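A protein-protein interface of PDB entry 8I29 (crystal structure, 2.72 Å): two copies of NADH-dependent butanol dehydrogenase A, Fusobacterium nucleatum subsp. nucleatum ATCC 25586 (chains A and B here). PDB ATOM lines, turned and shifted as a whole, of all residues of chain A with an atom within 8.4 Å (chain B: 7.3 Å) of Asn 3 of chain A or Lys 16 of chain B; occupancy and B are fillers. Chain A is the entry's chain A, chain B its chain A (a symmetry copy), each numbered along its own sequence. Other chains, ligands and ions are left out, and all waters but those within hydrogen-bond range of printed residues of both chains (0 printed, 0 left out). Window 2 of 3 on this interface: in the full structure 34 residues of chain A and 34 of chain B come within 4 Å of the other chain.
Among the printed residues, merely in contact across the chains: Asn 5 of chain A with Ile 13 of chain B, Asn 3 of chain A with Gly 15 of chain B, Asn 3 of chain A with Phe 14 of chain B, Asp 214 of chain A with Asn 244 of chain B, Asn 3 of chain A with Asn 18 of chain B, Asn 3 of chain A with Tyr 243 of chain B and Phe 4 of chain A with Ile 13 of chain B.
Asn 3 of chain A touches just these residues of chain B: Phe 14, Gly 15, Lys 16, Asn 18 and Tyr 243.
Lys 16 of chain B touches just one residue of chain A: Asn 3.
Of the printed residues of chain B, Asn 5 of chain A touches Ile 13.
Of the printed residues of chain A, Asn 244 of chain B touches Asp 214 (3.5 Å).
Printed residues of chain B within 4 Å of Asp 214 of chain A: Asn 244 (3.5 Å).
Printed residues of chain B within 4 Å of Phe 4 of chain A: Ile 13 (3.9 Å) and Phe 14 (2.9 Å).
Of the printed residues of chain A, Tyr 243 of chain B touches Asn 3.
Tyr 19 of chain B touches none of the printed residues of chain A.
The nearest residue of chain A that does not touch Lys 16 of chain B is Asp 2 of chain A (6.4 Å).
The backbone NH of Phe 14 of chain B is in hydrogen-bond range of the backbone carbonyl oxygen of Phe 4 of chain A.
The side-chain amide nitrogen of Asn 3 of chain A is in hydrogen-bond range of the backbone carbonyl oxygen of Lys 16 of chain B, at 2.6 Å.
Hydrophobic or aromatic side chains of chain B that line the printed part of chain A: Ile 13, Phe 14 and Tyr 243.
Of the 9 printed residues of chain A, 4 touch a printed residue of chain B.
Printed residues of chain A that touch a printed residue of chain B: Asn 3, Phe 4, Asn 5 and Asp 214.
Among the printed residues, 9 pairs touch across the chains.
Among the printed residues, no Asp or Glu carboxylate lies within 4 Å of a Lys or Arg side-chain nitrogen of the other chain.
The backbone NH of Leu 180 of chain B lies within hydrogen-bond range of the backbone carbonyl oxygen of Ile 13 of chain B (2.7 Å).
The backbone carbonyl oxygen (O) of Leu 180 of chain B is in hydrogen-bond range of the backbone NH (N) of Gly 15 of chain B, at 2.8 Å.
The backbone carbonyl oxygen of Gly 15 of chain B lies close to the side-chain amide oxygen of Asn 181 of chain B, 3.1 Å away.
No position is printed for both chains.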
ATOM      1  N   ASP A   2      -7.717  31.308  10.876  1.00  0.00           N
ATOM      2  CA  ASP A   2      -7.833  29.824  10.946  1.00  0.00           C
ATOM      3  C   ASP A   2      -6.794  29.186  10.024  1.00  0.00           C
ATOM      4  O   ASP A   2      -6.858  29.341   8.806  1.00  0.00           O
ATOM      5  CB  ASP A   2      -9.258  29.344  10.638  1.00  0.00           C
ATOM      6  CG  ASP A   2     -10.008  30.124   9.561  1.00  0.00           C
ATOM      7  OD1 ASP A   2      -9.359  30.949   8.853  1.00  0.00           O
ATOM      8  OD2 ASP A   2     -11.255  29.914   9.452  1.00  0.00           O
ATOM      9  N   ASN A   3      -5.815  28.508  10.643  1.00  0.00           N
ATOM     10  CA  ASN A   3      -4.766  27.754   9.971  1.00  0.00           C
ATOM     11  C   ASN A   3      -5.033  26.266  10.218  1.00  0.00           C
ATOM     12  O   ASN A   3      -5.794  25.894  11.110  1.00  0.00           O
ATOM     13  CB  ASN A   3      -3.375  28.139  10.492  1.00  0.00           C
ATOM     14  CG  ASN A   3      -2.865  29.525  10.121  1.00  0.00           C
ATOM     15  OD1 ASN A   3      -3.568  30.362   9.545  1.00  0.00           O
ATOM     16  ND2 ASN A   3      -1.597  29.766  10.412  1.00  0.00           N
ATOM     17  N   PHE A   4      -4.434  25.392   9.410  1.00  0.00           N
ATOM     18  CA  PHE A   4      -4.700  23.969   9.541  1.00  0.00           C
ATOM     19  C   PHE A   4      -3.553  23.182   8.929  1.00  0.00           C
ATOM     20  O   PHE A   4      -2.804  23.710   8.096  1.00  0.00           O
ATOM     21  CB  PHE A   4      -6.033  23.574   8.886  1.00  0.00           C
ATOM     22  CG  PHE A   4      -6.038  23.643   7.385  1.00  0.00           C
ATOM     23  CD1 PHE A   4      -6.327  24.831   6.732  1.00  0.00           C
ATOM     24  CD2 PHE A   4      -5.680  22.549   6.626  1.00  0.00           C
ATOM     25  CE1 PHE A   4      -6.291  24.918   5.350  1.00  0.00           C
ATOM     26  CE2 PHE A   4      -5.659  22.631   5.239  1.00  0.00           C
ATOM     27  CZ  PHE A   4      -5.959  23.816   4.602  1.00  0.00           C
ATOM     28  N   ASN A   5      -3.455  21.919   9.382  1.00  0.00           N
ATOM     29  CA  ASN A   5      -2.498  20.968   8.848  1.00  0.00           C
ATOM     30  C   ASN A   5      -3.236  19.761   8.251  1.00  0.00           C
ATOM     31  O   ASN A   5      -4.377  19.464   8.603  1.00  0.00           O
ATOM     32  CB  ASN A   5      -1.455  20.650   9.920  1.00  0.00           C
ATOM     33  CG  ASN A   5      -0.475  21.792  10.110  1.00  0.00           C
ATOM     34  OD1 ASN A   5      -0.829  22.970  10.037  1.00  0.00           O
ATOM     35  ND2 ASN A   5       0.792  21.463  10.271  1.00  0.00           N
ATOM     36  N   TYR A   6      -2.595  19.108   7.277  1.00  0.00           N
ATOM     37  CA  TYR A   6      -3.169  17.926   6.666  1.00  0.00           C
ATOM     38  C   TYR A   6      -2.086  16.963   6.183  1.00  0.00           C
ATOM     39  O   TYR A   6      -1.262  17.326   5.339  1.00  0.00           O
ATOM     40  CB  TYR A   6      -4.069  18.297   5.490  1.00  0.00           C
ATOM     41  CG  TYR A   6      -4.571  17.095   4.723  1.00  0.00           C
ATOM     42  CD1 TYR A   6      -5.628  16.316   5.196  1.00  0.00           C
ATOM     43  CD2 TYR A   6      -3.948  16.702   3.545  1.00  0.00           C
ATOM     44  CE1 TYR A   6      -6.073  15.201   4.497  1.00  0.00           C
ATOM     45  CE2 TYR A   6      -4.385  15.596   2.831  1.00  0.00           C
ATOM     46  CZ  TYR A   6      -5.451  14.844   3.306  1.00  0.00           C
ATOM     47  OH  TYR A   6      -5.858  13.744   2.578  1.00  0.00           O
ATOM     48  N   ASP A 214     -14.507  32.705   6.502  1.00  0.00           N
ATOM     49  CA  ASP A 214     -13.544  32.736   5.407  1.00  0.00           C
ATOM     50  C   ASP A 214     -13.314  31.333   4.838  1.00  0.00           C
ATOM     51  O   ASP A 214     -12.184  30.980   4.506  1.00  0.00           O
ATOM     52  CB  ASP A 214     -12.219  33.400   5.819  1.00  0.00           C
ATOM     53  CG  ASP A 214     -12.267  34.924   5.923  1.00  0.00           C
ATOM     54  OD1 ASP A 214     -13.360  35.503   5.652  1.00  0.00           O
ATOM     55  OD2 ASP A 214     -11.198  35.536   6.266  1.00  0.00           O
ATOM     56  N   CYS A 263     -11.304  22.365   6.159  1.00  0.00           N
ATOM     57  CA  CYS A 263      -9.935  22.858   6.309  1.00  0.00           C
ATOM     58  C   CYS A 263      -9.748  23.537   7.673  1.00  0.00           C
ATOM     59  O   CYS A 263      -9.652  24.764   7.744  1.00  0.00           O
ATOM     60  CB  CYS A 263      -9.583  23.917   5.259  1.00  0.00           C
ATOM     61  SG  CYS A 263      -9.744  23.465   3.502  1.00  0.00           S
ATOM     62  N   GLY A 264      -9.730  22.768   8.773  1.00  0.00           N
ATOM     63  CA  GLY A 264      -9.565  23.344  10.103  1.00  0.00           C
ATOM     64  C   GLY A 264     -10.746  24.205  10.578  1.00  0.00           C
ATOM     65  O   GLY A 264     -10.692  24.790  11.669  1.00  0.00           O
ATOM     66  N   ARG A 265     -11.799  24.309   9.754  1.00  0.00           N
ATOM     67  CA  ARG A 265     -13.096  24.781  10.218  1.00  0.00           C
ATOM     68  C   ARG A 265     -13.562  23.925  11.404  1.00  0.00           C
ATOM     69  O   ARG A 265     -13.193  22.746  11.503  1.00  0.00           O
ATOM     70  CB  ARG A 265     -14.109  24.695   9.074  1.00  0.00           C
ATOM     71  CG  ARG A 265     -14.439  23.264   8.680  1.00  0.00           C
ATOM     72  CD  ARG A 265     -15.191  23.215   7.377  1.00  0.00           C
ATOM     73  NE  ARG A 265     -16.494  23.830   7.508  1.00  0.00           N
ATOM     74  CZ  ARG A 265     -17.022  24.663   6.631  1.00  0.00           C
ATOM     75  NH1 ARG A 265     -18.251  25.109   6.796  1.00  0.00           N
ATOM     76  NH2 ARG A 265     -16.341  25.022   5.561  1.00  0.00           N
ATOM     77  N   ILE B  13       1.129  22.330   5.723  1.00  0.00           N
ATOM     78  CA  ILE B  13       0.962  23.345   6.756  1.00  0.00           C
ATOM     79  C   ILE B  13       0.436  24.623   6.105  1.00  0.00           C
ATOM     80  O   ILE B  13       1.204  25.371   5.490  1.00  0.00           O
ATOM     81  CB  ILE B  13       2.288  23.600   7.499  1.00  0.00           C
ATOM     82  CG1 ILE B  13       2.894  22.304   8.047  1.00  0.00           C
ATOM     83  CG2 ILE B  13       2.101  24.635   8.593  1.00  0.00           C
ATOM     84  CD1 ILE B  13       3.970  21.711   7.172  1.00  0.00           C
ATOM     85  N   PHE B  14      -0.874  24.863   6.278  1.00  0.00           N
ATOM     86  CA  PHE B  14      -1.572  25.956   5.614  1.00  0.00           C
ATOM     87  C   PHE B  14      -1.836  27.095   6.606  1.00  0.00           C
ATOM     88  O   PHE B  14      -2.390  26.880   7.687  1.00  0.00           O
ATOM     89  CB  PHE B  14      -2.908  25.485   5.015  1.00  0.00           C
ATOM     90  CG  PHE B  14      -3.514  26.506   4.090  1.00  0.00           C
ATOM     91  CD1 PHE B  14      -3.095  26.596   2.775  1.00  0.00           C
ATOM     92  CD2 PHE B  14      -4.428  27.440   4.557  1.00  0.00           C
ATOM     93  CE1 PHE B  14      -3.617  27.563   1.928  1.00  0.00           C
ATOM     94  CE2 PHE B  14      -4.934  28.417   3.711  1.00  0.00           C
ATOM     95  CZ  PHE B  14      -4.529  28.475   2.397  1.00  0.00           C
ATOM     96  N   GLY B  15      -1.493  28.324   6.203  1.00  0.00           N
ATOM     97  CA  GLY B  15      -1.772  29.474   7.046  1.00  0.00           C
ATOM     98  C   GLY B  15      -0.623  30.473   7.144  1.00  0.00           C
ATOM     99  O   GLY B  15       0.356  30.420   6.385  1.00  0.00           O
ATOM    100  N   LYS B  16      -0.791  31.404   8.084  1.00  0.00           N
ATOM    101  CA  LYS B  16       0.165  32.478   8.298  1.00  0.00           C
ATOM    102  C   LYS B  16       0.523  32.548   9.780  1.00  0.00           C
ATOM    103  O   LYS B  16      -0.201  31.978  10.599  1.00  0.00           O
ATOM    104  CB  LYS B  16      -0.448  33.817   7.872  1.00  0.00           C
ATOM    105  CG  LYS B  16      -1.638  34.266   8.724  1.00  0.00           C
ATOM    106  CD  LYS B  16      -2.161  35.653   8.384  1.00  0.00           C
ATOM    107  CE  LYS B  16      -3.488  35.969   9.038  1.00  0.00           C
ATOM    108  NZ  LYS B  16      -4.012  37.262   8.544  1.00  0.00           N
ATOM    109  N   ASP B  17       1.608  33.296  10.086  1.00  0.00           N
ATOM    110  CA  ASP B  17       2.066  33.601  11.441  1.00  0.00           C
ATOM    111  C   ASP B  17       2.376  32.287  12.152  1.00  0.00           C
ATOM    112  O   ASP B  17       1.892  32.026  13.246  1.00  0.00           O
ATOM    113  CB  ASP B  17       1.062  34.481  12.200  1.00  0.00           C
ATOM    114  CG  ASP B  17       0.783  35.819  11.533  1.00  0.00           C
ATOM    115  OD1 ASP B  17       1.623  36.260  10.703  1.00  0.00           O
ATOM    116  OD2 ASP B  17      -0.285  36.412  11.827  1.00  0.00           O
ATOM    117  N   ASN B  18       3.175  31.461  11.477  1.00  0.00           N
ATOM    118  CA  ASN B  18       3.434  30.090  11.871  1.00  0.00           C
ATOM    119  C   ASN B  18       4.808  29.718  11.313  1.00  0.00           C
ATOM    120  O   ASN B  18       4.989  28.669  10.687  1.00  0.00           O
ATOM    121  CB  ASN B  18       2.327  29.161  11.364  1.00  0.00           C
ATOM    122  CG  ASN B  18       2.302  29.004   9.850  1.00  0.00           C
ATOM    123  OD1 ASN B  18       2.969  29.728   9.096  1.00  0.00           O
ATOM    124  ND2 ASN B  18       1.539  28.023   9.392  1.00  0.00           N
ATOM    125  N   TYR B  19       5.778  30.617  11.512  1.00  0.00           N
ATOM    126  CA  TYR B  19       7.087  30.432  10.918  1.00  0.00           C
ATOM    127  C   TYR B  19       7.913  29.449  11.753  1.00  0.00           C
ATOM    128  O   TYR B  19       8.911  28.910  11.285  1.00  0.00           O
ATOM    129  CB  TYR B  19       7.708  31.804  10.656  1.00  0.00           C
ATOM    130  CG  TYR B  19       7.209  32.430   9.377  1.00  0.00           C
ATOM    131  CD1 TYR B  19       7.452  31.821   8.150  1.00  0.00           C
ATOM    132  CD2 TYR B  19       6.471  33.606   9.386  1.00  0.00           C
ATOM    133  CE1 TYR B  19       6.997  32.374   6.966  1.00  0.00           C
ATOM    134  CE2 TYR B  19       6.012  34.174   8.208  1.00  0.00           C
ATOM    135  CZ  TYR B  19       6.274  33.555   6.996  1.00  0.00           C
ATOM    136  OH  TYR B  19       5.821  34.103   5.825  1.00  0.00           O
ATOM    137  N   GLU B  21       6.949  26.533  12.341  1.00  0.00           N
ATOM    138  CA  GLU B  21       6.668  25.181  11.878  1.00  0.00           C
ATOM    139  C   GLU B  21       7.717  24.749  10.855  1.00  0.00           C
ATOM    140  O   GLU B  21       7.817  23.564  10.527  1.00  0.00           O
ATOM    141  CB  GLU B  21       5.217  25.020  11.414  1.00  0.00           C
ATOM    142  CG  GLU B  21       4.426  24.150  12.387  1.00  0.00           C
ATOM    143  CD  GLU B  21       2.927  24.374  12.474  1.00  0.00           C
ATOM    144  OE1 GLU B  21       2.417  25.138  11.630  1.00  0.00           O
ATOM    145  OE2 GLU B  21       2.276  23.800  13.411  1.00  0.00           O
ATOM    146  N   LEU B 180       2.468  26.499   3.366  1.00  0.00           N
ATOM    147  CA  LEU B 180       1.661  27.264   2.422  1.00  0.00           C
ATOM    148  C   LEU B 180       1.000  28.424   3.158  1.00  0.00           C
ATOM    149  O   LEU B 180      -0.019  28.250   3.830  1.00  0.00           O
ATOM    150  CB  LEU B 180       0.590  26.371   1.789  1.00  0.00           C
ATOM    151  CG  LEU B 180       1.050  25.224   0.883  1.00  0.00           C
ATOM    152  CD1 LEU B 180      -0.181  24.476   0.356  1.00  0.00           C
ATOM    153  CD2 LEU B 180       1.928  25.701  -0.279  1.00  0.00           C
ATOM    154  N   ASN B 181       1.632  29.594   3.035  1.00  0.00           N
ATOM    155  CA  ASN B 181       1.109  30.837   3.560  1.00  0.00           C
ATOM    156  C   ASN B 181       0.608  31.666   2.382  1.00  0.00           C
ATOM    157  O   ASN B 181       1.375  32.066   1.504  1.00  0.00           O
ATOM    158  CB  ASN B 181       2.158  31.596   4.377  1.00  0.00           C
ATOM    159  CG  ASN B 181       1.630  32.846   5.056  1.00  0.00           C
ATOM    160  OD1 ASN B 181       0.454  33.187   4.947  1.00  0.00           O
ATOM    161  ND2 ASN B 181       2.494  33.530   5.784  1.00  0.00           N
ATOM    162  N   PRO B 182      -0.705  31.966   2.350  1.00  0.00           N
ATOM    163  CA  PRO B 182      -1.282  32.799   1.297  1.00  0.00           C
ATOM    164  C   PRO B 182      -0.623  34.166   1.149  1.00  0.00           C
ATOM    165  O   PRO B 182      -0.665  34.745   0.067  1.00  0.00           O
ATOM    166  CB  PRO B 182      -2.710  33.016   1.775  1.00  0.00           C
ATOM    167  CG  PRO B 182      -2.993  31.817   2.635  1.00  0.00           C
ATOM    168  CD  PRO B 182      -1.692  31.536   3.349  1.00  0.00           C
ATOM    169  N   GLU B 183      -0.008  34.662   2.233  1.00  0.00           N
ATOM    170  CA  GLU B 183       0.588  35.990   2.261  1.00  0.00           C
ATOM    171  C   GLU B 183       1.665  36.135   1.199  1.00  0.00           C
ATOM    172  O   GLU B 183       1.937  37.248   0.791  1.00  0.00           O
ATOM    173  CB  GLU B 183       1.185  36.318   3.631  1.00  0.00           C
ATOM    174  CG  GLU B 183       0.125  36.555   4.711  1.00  0.00           C
ATOM    175  CD  GLU B 183       0.632  37.022   6.070  1.00  0.00           C
ATOM    176  OE1 GLU B 183       1.812  36.765   6.400  1.00  0.00           O
ATOM    177  OE2 GLU B 183      -0.158  37.673   6.789  1.00  0.00           O
ATOM    178  N   TYR B 186       0.829  38.276  -2.020  1.00  0.00           N
ATOM    179  CA  TYR B 186       0.686  39.732  -1.991  1.00  0.00           C
ATOM    180  C   TYR B 186       1.653  40.438  -2.945  1.00  0.00           C
ATOM    181  O   TYR B 186       1.289  41.347  -3.688  1.00  0.00           O
ATOM    182  CB  TYR B 186       0.939  40.239  -0.568  1.00  0.00           C
ATOM    183  CG  TYR B 186      -0.049  39.795   0.482  1.00  0.00           C
ATOM    184  CD1 TYR B 186      -1.135  38.991   0.173  1.00  0.00           C
ATOM    185  CD2 TYR B 186       0.079  40.209   1.799  1.00  0.00           C
ATOM    186  CE1 TYR B 186      -2.056  38.607   1.134  1.00  0.00           C
ATOM    187  CE2 TYR B 186      -0.825  39.824   2.779  1.00  0.00           C
ATOM    188  CZ  TYR B 186      -1.905  39.028   2.444  1.00  0.00           C
ATOM    189  OH  TYR B 186      -2.813  38.644   3.408  1.00  0.00           O
ATOM    190  N   TYR B 243      -6.253  38.594   2.593  1.00  0.00           N
ATOM    191  CA  TYR B 243      -5.826  37.264   3.010  1.00  0.00           C
ATOM    192  C   TYR B 243      -6.851  36.193   2.619  1.00  0.00           C
ATOM    193  O   TYR B 243      -6.473  35.133   2.149  1.00  0.00           O
ATOM    194  CB  TYR B 243      -5.574  37.219   4.518  1.00  0.00           C
ATOM    195  CG  TYR B 243      -5.060  35.883   4.974  1.00  0.00           C
ATOM    196  CD1 TYR B 243      -3.765  35.488   4.684  1.00  0.00           C
ATOM    197  CD2 TYR B 243      -5.899  34.969   5.590  1.00  0.00           C
ATOM    198  CE1 TYR B 243      -3.306  34.234   5.050  1.00  0.00           C
ATOM    199  CE2 TYR B 243      -5.445  33.723   5.981  1.00  0.00           C
ATOM    200  CZ  TYR B 243      -4.148  33.352   5.700  1.00  0.00           C
ATOM    201  OH  TYR B 243      -3.743  32.105   6.087  1.00  0.00           O
ATOM    202  N   ASN B 244      -8.140  36.491   2.814  1.00  0.00           N
ATOM    203  CA  ASN B 244      -9.241  35.613   2.451  1.00  0.00           C
ATOM    204  C   ASN B 244      -9.162  35.265   0.968  1.00  0.00           C
ATOM    205  O   ASN B 244      -9.127  34.089   0.627  1.00  0.00           O
ATOM    206  CB  ASN B 244     -10.589  36.238   2.836  1.00  0.00           C
ATOM    207  CG  ASN B 244     -11.811  35.454   2.401  1.00  0.00           C
ATOM    208  OD1 ASN B 244     -11.875  34.224   2.453  1.00  0.00           O
ATOM    209  ND2 ASN B 244     -12.814  36.181   1.968  1.00  0.00           N
